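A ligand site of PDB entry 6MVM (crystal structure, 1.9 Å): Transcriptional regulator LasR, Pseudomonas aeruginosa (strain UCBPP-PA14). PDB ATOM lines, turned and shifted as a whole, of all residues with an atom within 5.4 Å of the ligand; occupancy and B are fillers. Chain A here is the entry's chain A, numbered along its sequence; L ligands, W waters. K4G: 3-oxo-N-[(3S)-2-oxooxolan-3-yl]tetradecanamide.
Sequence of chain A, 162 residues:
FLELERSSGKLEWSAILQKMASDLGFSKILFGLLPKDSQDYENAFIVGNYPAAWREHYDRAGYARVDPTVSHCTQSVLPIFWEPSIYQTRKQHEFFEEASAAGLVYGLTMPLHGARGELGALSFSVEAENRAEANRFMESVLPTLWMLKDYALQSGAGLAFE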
ATOM      1  N   LEU A  30      -0.182 -23.434  22.962  1.00  0.00           N
ATOM      2  CA  LEU A  30      -0.870 -22.626  21.973  1.00  0.00           C
ATOM      3  C   LEU A  30       0.071 -21.549  21.462  1.00  0.00           C
ATOM      4  O   LEU A  30       0.736 -20.886  22.254  1.00  0.00           O
ATOM      5  CB  LEU A  30      -2.151 -21.996  22.543  1.00  0.00           C
ATOM      6  CG  LEU A  30      -3.024 -21.230  21.536  1.00  0.00           C
ATOM      7  CD1 LEU A  30      -4.481 -21.444  21.835  1.00  0.00           C
ATOM      8  CD2 LEU A  30      -2.702 -19.726  21.503  1.00  0.00           C
ATOM      9  N   GLY A  32      -0.461 -18.304  19.083  1.00  0.00           N
ATOM     10  CA  GLY A  32      -1.376 -17.458  18.334  1.00  0.00           C
ATOM     11  C   GLY A  32      -0.669 -16.223  17.831  1.00  0.00           C
ATOM     12  O   GLY A  32       0.144 -15.659  18.547  1.00  0.00           O
ATOM     13  N   LEU A  33      -0.965 -15.803  16.603  1.00  0.00           N
ATOM     14  CA  LEU A  33      -0.319 -14.634  16.033  1.00  0.00           C
ATOM     15  C   LEU A  33      -1.244 -13.872  15.078  1.00  0.00           C
ATOM     16  O   LEU A  33      -1.851 -14.461  14.212  1.00  0.00           O
ATOM     17  CB  LEU A  33       0.953 -15.059  15.296  1.00  0.00           C
ATOM     18  CG  LEU A  33       2.082 -14.038  15.135  1.00  0.00           C
ATOM     19  CD1 LEU A  33       2.679 -13.673  16.493  1.00  0.00           C
ATOM     20  CD2 LEU A  33       3.154 -14.558  14.193  1.00  0.00           C
ATOM     21  N   LEU A  34      -1.322 -12.556  15.273  1.00  0.00           N
ATOM     22  CA  LEU A  34      -2.038 -11.642  14.370  1.00  0.00           C
ATOM     23  C   LEU A  34      -1.072 -10.702  13.670  1.00  0.00           C
ATOM     24  O   LEU A  34      -0.140 -10.207  14.302  1.00  0.00           O
ATOM     25  CB  LEU A  34      -3.066 -10.793  15.127  1.00  0.00           C
ATOM     26  CG  LEU A  34      -4.090 -11.407  16.068  1.00  0.00           C
ATOM     27  CD1 LEU A  34      -4.368 -10.412  17.167  1.00  0.00           C
ATOM     28  CD2 LEU A  34      -5.370 -11.744  15.326  1.00  0.00           C
ATOM     29  N   TYR A  41      -9.287 -11.675  15.729  1.00  0.00           N
ATOM     30  CA  TYR A  41      -8.893 -12.883  16.449  1.00  0.00           C
ATOM     31  C   TYR A  41      -9.501 -14.146  15.838  1.00  0.00           C
ATOM     32  O   TYR A  41      -9.030 -15.259  16.088  1.00  0.00           O
ATOM     33  CB  TYR A  41      -9.322 -12.813  17.915  1.00  0.00           C
ATOM     34  CG  TYR A  41      -8.663 -11.722  18.733  1.00  0.00           C
ATOM     35  CD1 TYR A  41      -7.868 -10.754  18.149  1.00  0.00           C
ATOM     36  CD2 TYR A  41      -8.834 -11.683  20.099  1.00  0.00           C
ATOM     37  CE1 TYR A  41      -7.275  -9.765  18.894  1.00  0.00           C
ATOM     38  CE2 TYR A  41      -8.248 -10.707  20.864  1.00  0.00           C
ATOM     39  CZ  TYR A  41      -7.460  -9.740  20.256  1.00  0.00           C
ATOM     40  OH  TYR A  41      -6.881  -8.758  21.026  1.00  0.00           O
ATOM     41  N   ALA A  44      -7.091 -15.340  13.449  1.00  0.00           N
ATOM     42  CA  ALA A  44      -5.779 -15.479  14.078  1.00  0.00           C
ATOM     43  C   ALA A  44      -5.149 -16.824  13.752  1.00  0.00           C
ATOM     44  O   ALA A  44      -5.815 -17.856  13.838  1.00  0.00           O
ATOM     45  CB  ALA A  44      -5.867 -15.297  15.572  1.00  0.00           C
ATOM     46  N   PHE A  45      -3.884 -16.792  13.340  1.00  0.00           N
ATOM     47  CA  PHE A  45      -3.052 -17.978  13.123  1.00  0.00           C
ATOM     48  C   PHE A  45      -2.878 -18.714  14.449  1.00  0.00           C
ATOM     49  O   PHE A  45      -2.301 -18.168  15.374  1.00  0.00           O
ATOM     50  CB  PHE A  45      -1.694 -17.572  12.560  1.00  0.00           C
ATOM     51  CG  PHE A  45      -0.746 -18.707  12.307  1.00  0.00           C
ATOM     52  CD1 PHE A  45       0.196 -19.070  13.251  1.00  0.00           C
ATOM     53  CD2 PHE A  45      -0.787 -19.405  11.110  1.00  0.00           C
ATOM     54  CE1 PHE A  45       1.071 -20.121  13.014  1.00  0.00           C
ATOM     55  CE2 PHE A  45       0.085 -20.452  10.864  1.00  0.00           C
ATOM     56  CZ  PHE A  45       1.020 -20.809  11.814  1.00  0.00           C
ATOM     57  N   ILE A  46      -3.409 -19.929  14.560  1.00  0.00           N
ATOM     58  CA  ILE A  46      -3.366 -20.623  15.836  1.00  0.00           C
ATOM     59  C   ILE A  46      -2.684 -21.979  15.693  1.00  0.00           C
ATOM     60  O   ILE A  46      -2.985 -22.725  14.757  1.00  0.00           O
ATOM     61  CB  ILE A  46      -4.786 -20.820  16.437  1.00  0.00           C
ATOM     62  CG1 ILE A  46      -5.513 -19.489  16.569  1.00  0.00           C
ATOM     63  CG2 ILE A  46      -4.709 -21.527  17.803  1.00  0.00           C
ATOM     64  CD1 ILE A  46      -4.865 -18.532  17.519  1.00  0.00           C
ATOM     65  N   TYR A  50      -4.255 -27.518  22.396  1.00  0.00           N
ATOM     66  CA  TYR A  50      -5.352 -27.279  23.301  1.00  0.00           C
ATOM     67  C   TYR A  50      -6.505 -28.163  22.882  1.00  0.00           C
ATOM     68  O   TYR A  50      -6.664 -28.428  21.681  1.00  0.00           O
ATOM     69  CB  TYR A  50      -5.790 -25.813  23.287  1.00  0.00           C
ATOM     70  CG  TYR A  50      -4.965 -24.950  24.191  1.00  0.00           C
ATOM     71  CD1 TYR A  50      -3.779 -25.416  24.741  1.00  0.00           C
ATOM     72  CD2 TYR A  50      -5.378 -23.664  24.524  1.00  0.00           C
ATOM     73  CE1 TYR A  50      -3.019 -24.630  25.585  1.00  0.00           C
ATOM     74  CE2 TYR A  50      -4.618 -22.879  25.368  1.00  0.00           C
ATOM     75  CZ  TYR A  50      -3.443 -23.371  25.894  1.00  0.00           C
ATOM     76  OH  TYR A  50      -2.690 -22.592  26.736  1.00  0.00           O
ATOM     77  N   TRP A  54     -12.433 -26.869  23.803  1.00  0.00           N
ATOM     78  CA  TRP A  54     -12.059 -25.649  24.485  1.00  0.00           C
ATOM     79  C   TRP A  54     -11.763 -24.541  23.480  1.00  0.00           C
ATOM     80  O   TRP A  54     -12.253 -23.432  23.614  1.00  0.00           O
ATOM     81  CB  TRP A  54     -10.844 -25.885  25.382  1.00  0.00           C
ATOM     82  CG  TRP A  54     -10.314 -24.637  26.024  1.00  0.00           C
ATOM     83  CD1 TRP A  54      -9.083 -24.060  25.804  1.00  0.00           C
ATOM     84  CD2 TRP A  54     -10.992 -23.794  26.969  1.00  0.00           C
ATOM     85  NE1 TRP A  54      -8.955 -22.930  26.569  1.00  0.00           N
ATOM     86  CE2 TRP A  54     -10.103 -22.739  27.293  1.00  0.00           C
ATOM     87  CE3 TRP A  54     -12.248 -23.825  27.573  1.00  0.00           C
ATOM     88  CZ2 TRP A  54     -10.453 -21.726  28.197  1.00  0.00           C
ATOM     89  CZ3 TRP A  54     -12.592 -22.829  28.465  1.00  0.00           C
ATOM     90  CH2 TRP A  54     -11.697 -21.791  28.776  1.00  0.00           C
ATOM     91  N   ARG A  55     -10.963 -24.844  22.461  1.00  0.00           N
ATOM     92  CA  ARG A  55     -10.639 -23.837  21.459  1.00  0.00           C
ATOM     93  C   ARG A  55     -11.884 -23.221  20.825  1.00  0.00           C
ATOM     94  O   ARG A  55     -11.941 -22.010  20.595  1.00  0.00           O
ATOM     95  CB  ARG A  55      -9.744 -24.446  20.369  1.00  0.00           C
ATOM     96  CG  ARG A  55      -8.256 -24.572  20.759  1.00  0.00           C
ATOM     97  CD  ARG A  55      -7.421 -23.338  20.392  1.00  0.00           C
ATOM     98  NE  ARG A  55      -7.890 -22.118  21.048  1.00  0.00           N
ATOM     99  CZ  ARG A  55      -8.464 -21.109  20.407  1.00  0.00           C
ATOM    100  NH1 ARG A  55      -8.636 -21.178  19.098  1.00  0.00           N
ATOM    101  NH2 ARG A  55      -8.863 -20.030  21.063  1.00  0.00           N
ATOM    102  N   TYR A  58     -13.925 -21.233  23.617  1.00  0.00           N
ATOM    103  CA  TYR A  58     -13.103 -20.041  23.767  1.00  0.00           C
ATOM    104  C   TYR A  58     -13.439 -19.004  22.691  1.00  0.00           C
ATOM    105  O   TYR A  58     -13.775 -17.873  22.990  1.00  0.00           O
ATOM    106  CB  TYR A  58     -11.612 -20.424  23.672  1.00  0.00           C
ATOM    107  CG  TYR A  58     -10.637 -19.376  24.143  1.00  0.00           C
ATOM    108  CD1 TYR A  58     -10.355 -18.252  23.361  1.00  0.00           C
ATOM    109  CD2 TYR A  58      -9.977 -19.496  25.359  1.00  0.00           C
ATOM    110  CE1 TYR A  58      -9.462 -17.296  23.784  1.00  0.00           C
ATOM    111  CE2 TYR A  58      -9.071 -18.538  25.778  1.00  0.00           C
ATOM    112  CZ  TYR A  58      -8.824 -17.449  24.987  1.00  0.00           C
ATOM    113  OH  TYR A  58      -7.944 -16.478  25.398  1.00  0.00           O
ATOM    114  N   ALA A  64     -11.223 -14.155  24.506  1.00  0.00           N
ATOM    115  CA  ALA A  64      -9.963 -13.497  24.300  1.00  0.00           C
ATOM    116  C   ALA A  64     -10.039 -12.129  24.976  1.00  0.00           C
ATOM    117  O   ALA A  64      -9.026 -11.571  25.372  1.00  0.00           O
ATOM    118  CB  ALA A  64      -9.649 -13.368  22.836  1.00  0.00           C
ATOM    119  N   ASP A  67      -9.833 -13.387  29.029  1.00  0.00           N
ATOM    120  CA  ASP A  67      -8.511 -13.948  29.302  1.00  0.00           C
ATOM    121  C   ASP A  67      -7.486 -12.886  29.691  1.00  0.00           C
ATOM    122  O   ASP A  67      -7.035 -12.114  28.844  1.00  0.00           O
ATOM    123  CB  ASP A  67      -8.018 -14.691  28.057  1.00  0.00           C
ATOM    124  CG  ASP A  67      -6.968 -15.736  28.371  1.00  0.00           C
ATOM    125  OD1 ASP A  67      -6.335 -15.693  29.437  1.00  0.00           O
ATOM    126  OD2 ASP A  67      -6.787 -16.620  27.507  1.00  0.00           O
ATOM    127  N   THR A  69      -4.417 -13.351  30.199  1.00  0.00           N
ATOM    128  CA  THR A  69      -3.131 -13.581  29.549  1.00  0.00           C
ATOM    129  C   THR A  69      -3.088 -12.835  28.236  1.00  0.00           C
ATOM    130  O   THR A  69      -2.036 -12.415  27.803  1.00  0.00           O
ATOM    131  CB  THR A  69      -2.815 -15.075  29.296  1.00  0.00           C
ATOM    132  OG1 THR A  69      -3.814 -15.669  28.459  1.00  0.00           O
ATOM    133  CG2 THR A  69      -2.727 -15.854  30.616  1.00  0.00           C
ATOM    134  N   VAL A  70      -4.241 -12.655  27.612  1.00  0.00           N
ATOM    135  CA  VAL A  70      -4.260 -11.939  26.327  1.00  0.00           C
ATOM    136  C   VAL A  70      -4.047 -10.444  26.536  1.00  0.00           C
ATOM    137  O   VAL A  70      -3.215  -9.820  25.866  1.00  0.00           O
ATOM    138  CB  VAL A  70      -5.569 -12.188  25.576  1.00  0.00           C
ATOM    139  CG1 VAL A  70      -5.610 -11.353  24.297  1.00  0.00           C
ATOM    140  CG2 VAL A  70      -5.740 -13.689  25.275  1.00  0.00           C
ATOM    141  N   CYS A  73      -0.459  -9.679  27.215  1.00  0.00           N
ATOM    142  CA  CYS A  73       0.442  -9.717  26.050  1.00  0.00           C
ATOM    143  C   CYS A  73       0.365  -8.440  25.221  1.00  0.00           C
ATOM    144  O   CYS A  73       1.302  -8.119  24.490  1.00  0.00           O
ATOM    145  CB  CYS A  73       0.123 -10.925  25.148  1.00  0.00           C
ATOM    146  SG  CYS A  73       0.476 -12.549  25.867  1.00  0.00           S
ATOM    147  N   THR A  74      -0.748  -7.719  25.322  1.00  0.00           N
ATOM    148  CA  THR A  74      -0.886  -6.474  24.580  1.00  0.00           C
ATOM    149  C   THR A  74      -0.074  -5.391  25.278  1.00  0.00           C
ATOM    150  O   THR A  74       0.292  -4.402  24.653  1.00  0.00           O
ATOM    151  CB  THR A  74      -2.373  -6.015  24.463  1.00  0.00           C
ATOM    152  OG1 THR A  74      -2.807  -5.411  25.689  1.00  0.00           O
ATOM    153  CG2 THR A  74      -3.263  -7.194  24.126  1.00  0.00           C
ATOM    154  N   TRP A  82       0.136 -18.348  35.155  1.00  0.00           N
ATOM    155  CA  TRP A  82      -1.292 -18.450  35.401  1.00  0.00           C
ATOM    156  C   TRP A  82      -1.519 -18.646  36.903  1.00  0.00           C
ATOM    157  O   TRP A  82      -1.495 -19.776  37.400  1.00  0.00           O
ATOM    158  CB  TRP A  82      -1.924 -19.600  34.598  1.00  0.00           C
ATOM    159  CG  TRP A  82      -1.667 -19.576  33.092  1.00  0.00           C
ATOM    160  CD1 TRP A  82      -1.137 -18.551  32.356  1.00  0.00           C
ATOM    161  CD2 TRP A  82      -1.906 -20.644  32.172  1.00  0.00           C
ATOM    162  NE1 TRP A  82      -1.034 -18.919  31.037  1.00  0.00           N
ATOM    163  CE2 TRP A  82      -1.509 -20.199  30.893  1.00  0.00           C
ATOM    164  CE3 TRP A  82      -2.422 -21.949  32.296  1.00  0.00           C
ATOM    165  CZ2 TRP A  82      -1.609 -21.008  29.749  1.00  0.00           C
ATOM    166  CZ3 TRP A  82      -2.515 -22.751  31.153  1.00  0.00           C
ATOM    167  CH2 TRP A  82      -2.117 -22.269  29.896  1.00  0.00           C
ATOM    168  N   TYR A  87      -6.674 -13.730  37.751  1.00  0.00           N
ATOM    169  CA  TYR A  87      -8.098 -13.859  37.443  1.00  0.00           C
ATOM    170  C   TYR A  87      -8.911 -13.073  38.463  1.00  0.00           C
ATOM    171  O   TYR A  87      -9.206 -13.597  39.536  1.00  0.00           O
ATOM    172  CB  TYR A  87      -8.535 -15.333  37.474  1.00  0.00           C
ATOM    173  CG  TYR A  87      -7.858 -16.232  36.471  1.00  0.00           C
ATOM    174  CD1 TYR A  87      -8.166 -16.156  35.115  1.00  0.00           C
ATOM    175  CD2 TYR A  87      -6.929 -17.179  36.875  1.00  0.00           C
ATOM    176  CE1 TYR A  87      -7.547 -16.989  34.198  1.00  0.00           C
ATOM    177  CE2 TYR A  87      -6.314 -18.012  35.971  1.00  0.00           C
ATOM    178  CZ  TYR A  87      -6.619 -17.916  34.638  1.00  0.00           C
ATOM    179  OH  TYR A  87      -6.017 -18.750  33.738  1.00  0.00           O
ATOM    180  N   PHE A  95     -14.120 -17.937  33.801  1.00  0.00           N
ATOM    181  CA  PHE A  95     -13.190 -18.345  32.745  1.00  0.00           C
ATOM    182  C   PHE A  95     -12.145 -19.293  33.326  1.00  0.00           C
ATOM    183  O   PHE A  95     -11.871 -20.356  32.762  1.00  0.00           O
ATOM    184  CB  PHE A  95     -12.508 -17.127  32.119  1.00  0.00           C
ATOM    185  CG  PHE A  95     -11.362 -17.483  31.200  1.00  0.00           C
ATOM    186  CD1 PHE A  95     -10.050 -17.467  31.665  1.00  0.00           C
ATOM    187  CD2 PHE A  95     -11.594 -17.815  29.865  1.00  0.00           C
ATOM    188  CE1 PHE A  95      -8.984 -17.789  30.819  1.00  0.00           C
ATOM    189  CE2 PHE A  95     -10.542 -18.139  29.024  1.00  0.00           C
ATOM    190  CZ  PHE A  95      -9.240 -18.130  29.500  1.00  0.00           C
ATOM    191  N   ALA A  99     -11.588 -23.104  32.160  1.00  0.00           N
ATOM    192  CA  ALA A  99     -10.270 -23.369  31.636  1.00  0.00           C
ATOM    193  C   ALA A  99      -9.621 -24.480  32.445  1.00  0.00           C
ATOM    194  O   ALA A  99      -8.973 -25.362  31.903  1.00  0.00           O
ATOM    195  CB  ALA A  99      -9.430 -22.118  31.644  1.00  0.00           C
ATOM    196  N   LEU A 104      -6.420 -26.785  31.875  1.00  0.00           N
ATOM    197  CA  LEU A 104      -5.480 -25.670  31.802  1.00  0.00           C
ATOM    198  C   LEU A 104      -5.439 -24.905  33.136  1.00  0.00           C
ATOM    199  O   LEU A 104      -5.938 -23.793  33.238  1.00  0.00           O
ATOM    200  CB  LEU A 104      -5.852 -24.737  30.653  1.00  0.00           C
ATOM    201  CG  LEU A 104      -5.944 -25.463  29.312  1.00  0.00           C
ATOM    202  CD1 LEU A 104      -6.572 -24.586  28.258  1.00  0.00           C
ATOM    203  CD2 LEU A 104      -4.556 -25.917  28.869  1.00  0.00           C
ATOM    204  N   THR A 109       2.230 -17.770  29.867  1.00  0.00           N
ATOM    205  CA  THR A 109       2.138 -17.251  28.515  1.00  0.00           C
ATOM    206  C   THR A 109       3.296 -16.278  28.254  1.00  0.00           C
ATOM    207  O   THR A 109       3.551 -15.367  29.049  1.00  0.00           O
ATOM    208  CB  THR A 109       0.809 -16.531  28.266  1.00  0.00           C
ATOM    209  OG1 THR A 109      -0.277 -17.379  28.661  1.00  0.00           O
ATOM    210  CG2 THR A 109       0.655 -16.192  26.792  1.00  0.00           C
ATOM    211  N   LEU A 119       1.632  -9.492  16.484  1.00  0.00           N
ATOM    212  CA  LEU A 119       1.204  -9.590  17.872  1.00  0.00           C
ATOM    213  C   LEU A 119       0.728 -10.997  18.140  1.00  0.00           C
ATOM    214  O   LEU A 119      -0.006 -11.561  17.335  1.00  0.00           O
ATOM    215  CB  LEU A 119       0.092  -8.593  18.187  1.00  0.00           C
ATOM    216  CG  LEU A 119      -0.592  -8.678  19.566  1.00  0.00           C
ATOM    217  CD1 LEU A 119       0.326  -8.178  20.706  1.00  0.00           C
ATOM    218  CD2 LEU A 119      -1.907  -7.913  19.546  1.00  0.00           C
ATOM    219  N   GLY A 120       1.137 -11.563  19.277  1.00  0.00           N
ATOM    220  CA  GLY A 120       0.778 -12.939  19.582  1.00  0.00           C
ATOM    221  C   GLY A 120       1.043 -13.375  21.007  1.00  0.00           C
ATOM    222  O   GLY A 120       1.277 -12.571  21.917  1.00  0.00           O
ATOM    223  N   ALA A 121       0.999 -14.692  21.197  1.00  0.00           N
ATOM    224  CA  ALA A 121       1.170 -15.278  22.505  1.00  0.00           C
ATOM    225  C   ALA A 121       1.578 -16.729  22.343  1.00  0.00           C
ATOM    226  O   ALA A 121       1.050 -17.428  21.492  1.00  0.00           O
ATOM    227  CB  ALA A 121      -0.132 -15.186  23.322  1.00  0.00           C
ATOM    228  N   SER A 123       1.639 -19.934  24.830  1.00  0.00           N
ATOM    229  CA  SER A 123       1.310 -20.484  26.144  1.00  0.00           C
ATOM    230  C   SER A 123       1.797 -21.892  26.308  1.00  0.00           C
ATOM    231  O   SER A 123       1.696 -22.695  25.376  1.00  0.00           O
ATOM    232  CB  SER A 123      -0.205 -20.454  26.378  1.00  0.00           C
ATOM    233  OG  SER A 123      -0.710 -19.143  26.394  1.00  0.00           O
HETATM  234  C10 K4G L   1      -5.985 -17.661  22.275  1.00  0.00           C
HETATM  235  C15 K4G L   1      -4.132 -18.901  26.771  1.00  0.00           C
HETATM  236  C20 K4G L   1      -6.042 -20.341  30.976  1.00  0.00           C
HETATM  237  C22 K4G L   1      -6.184 -20.801  28.738  1.00  0.00           C
HETATM  238  C01 K4G L   1      -2.282 -10.892  22.411  1.00  0.00           C
HETATM  239  C02 K4G L   1      -2.406 -12.116  21.539  1.00  0.00           C
HETATM  240  C03 K4G L   1      -3.633 -12.081  20.636  1.00  0.00           C
HETATM  241  C04 K4G L   1      -3.412 -12.936  19.372  1.00  0.00           C
HETATM  242  C05 K4G L   1      -3.448 -14.428  19.663  1.00  0.00           C
HETATM  243  C06 K4G L   1      -4.678 -15.140  19.081  1.00  0.00           C
HETATM  244  C07 K4G L   1      -5.987 -14.697  19.721  1.00  0.00           C
HETATM  245  C08 K4G L   1      -6.553 -15.703  20.762  1.00  0.00           C
HETATM  246  C09 K4G L   1      -5.734 -16.997  20.924  1.00  0.00           C
HETATM  247  C11 K4G L   1      -4.980 -17.263  23.360  1.00  0.00           C
HETATM  248  C12 K4G L   1      -5.047 -18.123  24.589  1.00  0.00           C
HETATM  249  C14 K4G L   1      -4.222 -17.745  25.787  1.00  0.00           C
HETATM  250  C18 K4G L   1      -4.906 -19.957  28.869  1.00  0.00           C
HETATM  251  C19 K4G L   1      -5.003 -19.469  30.319  1.00  0.00           C
HETATM  252  N17 K4G L   1      -4.956 -18.871  27.891  1.00  0.00           N
HETATM  253  O13 K4G L   1      -5.741 -19.132  24.637  1.00  0.00           O
HETATM  254  O16 K4G L   1      -3.350 -19.829  26.579  1.00  0.00           O
HETATM  255  O21 K4G L   1      -6.627 -21.163  29.974  1.00  0.00           O
HETATM  256  O23 K4G L   1      -6.803 -21.169  27.777  1.00  0.00           O
HETATM  257  O   HOH W   1      -7.552 -20.798  24.059  1.00  0.00           O
HETATM  258  O   HOH W   2      -9.860 -16.361  20.667  1.00  0.00           O
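N of Ser 123 is in hydrogen-bond range of O of Leu 30.
The side-chain hydroxyl of Thr 109 is in hydrogen-bond range of the side-chain hydroxyl of Ser 123 (2.9 Å).
The side-chain hydroxyl of Thr 69 is in hydrogen-bond range of the side-chain carboxylate of Asp 67.
OH of Tyr 58 sits at hydrogen-bond distance from OD2 of Asp 67.
O of Ala 99 is in hydrogen-bond range of N of Leu 104 (2.9 Å).
The backbone carbonyl oxygen (O) of Thr 69 lies within hydrogen-bond range of the side-chain sulfur (SG) of Cys 73 (3.2 Å).
The backbone NH (N) of Leu 34 is in hydrogen-bond range of the backbone carbonyl oxygen (O) of Leu 119.
NE1 of Trp 82 sits at hydrogen-bond distance from OG1 of Thr 109 (2.9 Å).
Water W1 bridges O13 of the ligand and NE of Arg 55.
O16 of the ligand sits at hydrogen-bond distance from OG of Ser 123 (2.7 Å).
The side-chain hydroxyl (OH) of Tyr 50 is in hydrogen-bond range of an oxygen (O16) of the ligand (2.8 Å).
A nitrogen (N17) of the ligand lies within hydrogen-bond range of the side-chain carboxylate (OD2) of Asp 67.
O23 of the ligand lies within hydrogen-bond range of NE1 of Trp 54 (3.0 Å).
A nitrogen (N17) of the ligand lies close to the side-chain hydroxyl of Thr 69, at 3.4 Å.
Leu 30 touches the ligand (CD2 to C11, 3.8 Å).
Gly 32 touches the ligand (C to C05, 3.8 Å).
CD1 of Leu 34 touches C04 of the ligand, at 3.5 Å.
Ala 44 touches the ligand (CB to C06, 3.7 Å).
Ile 46 touches the ligand (CD1 to C06, 3.7 Å).
Arg 55 touches the ligand (NH2 to C10, 3.9 Å).
OH of Tyr 58 touches C12 of the ligand (3.4 Å).
Val 70 touches the ligand (O to C01, 3.7 Å).
CB of Cys 73 touches C01 of the ligand (3.6 Å).
Trp 82 touches the ligand.
Tyr 87 touches the ligand.
Phe 95 touches the ligand (CE1 to C20, 3.9 Å).
CB of Ala 99 touches O21 of the ligand (3.4 Å).
Leu 104 touches the ligand.
Leu 119 touches the ligand (CG to C01, 3.98 Å).
C of Gly 120 touches C02 of the ligand, at 3.7 Å.
Within 4 Å of the ligand: Leu 30, Gly 32, Leu 34, Ala 44, Ile 46, Tyr 50, Trp 54, Arg 55, Tyr 58, Asp 67, Thr 69, Val 70, Cys 73, Trp 82, Tyr 87, Phe 95, Ala 99, Leu 104, Leu 119, Gly 120 and Ser 123.
The nearest printed residue that does not touch the ligand is Tyr 41 (4.1 Å).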
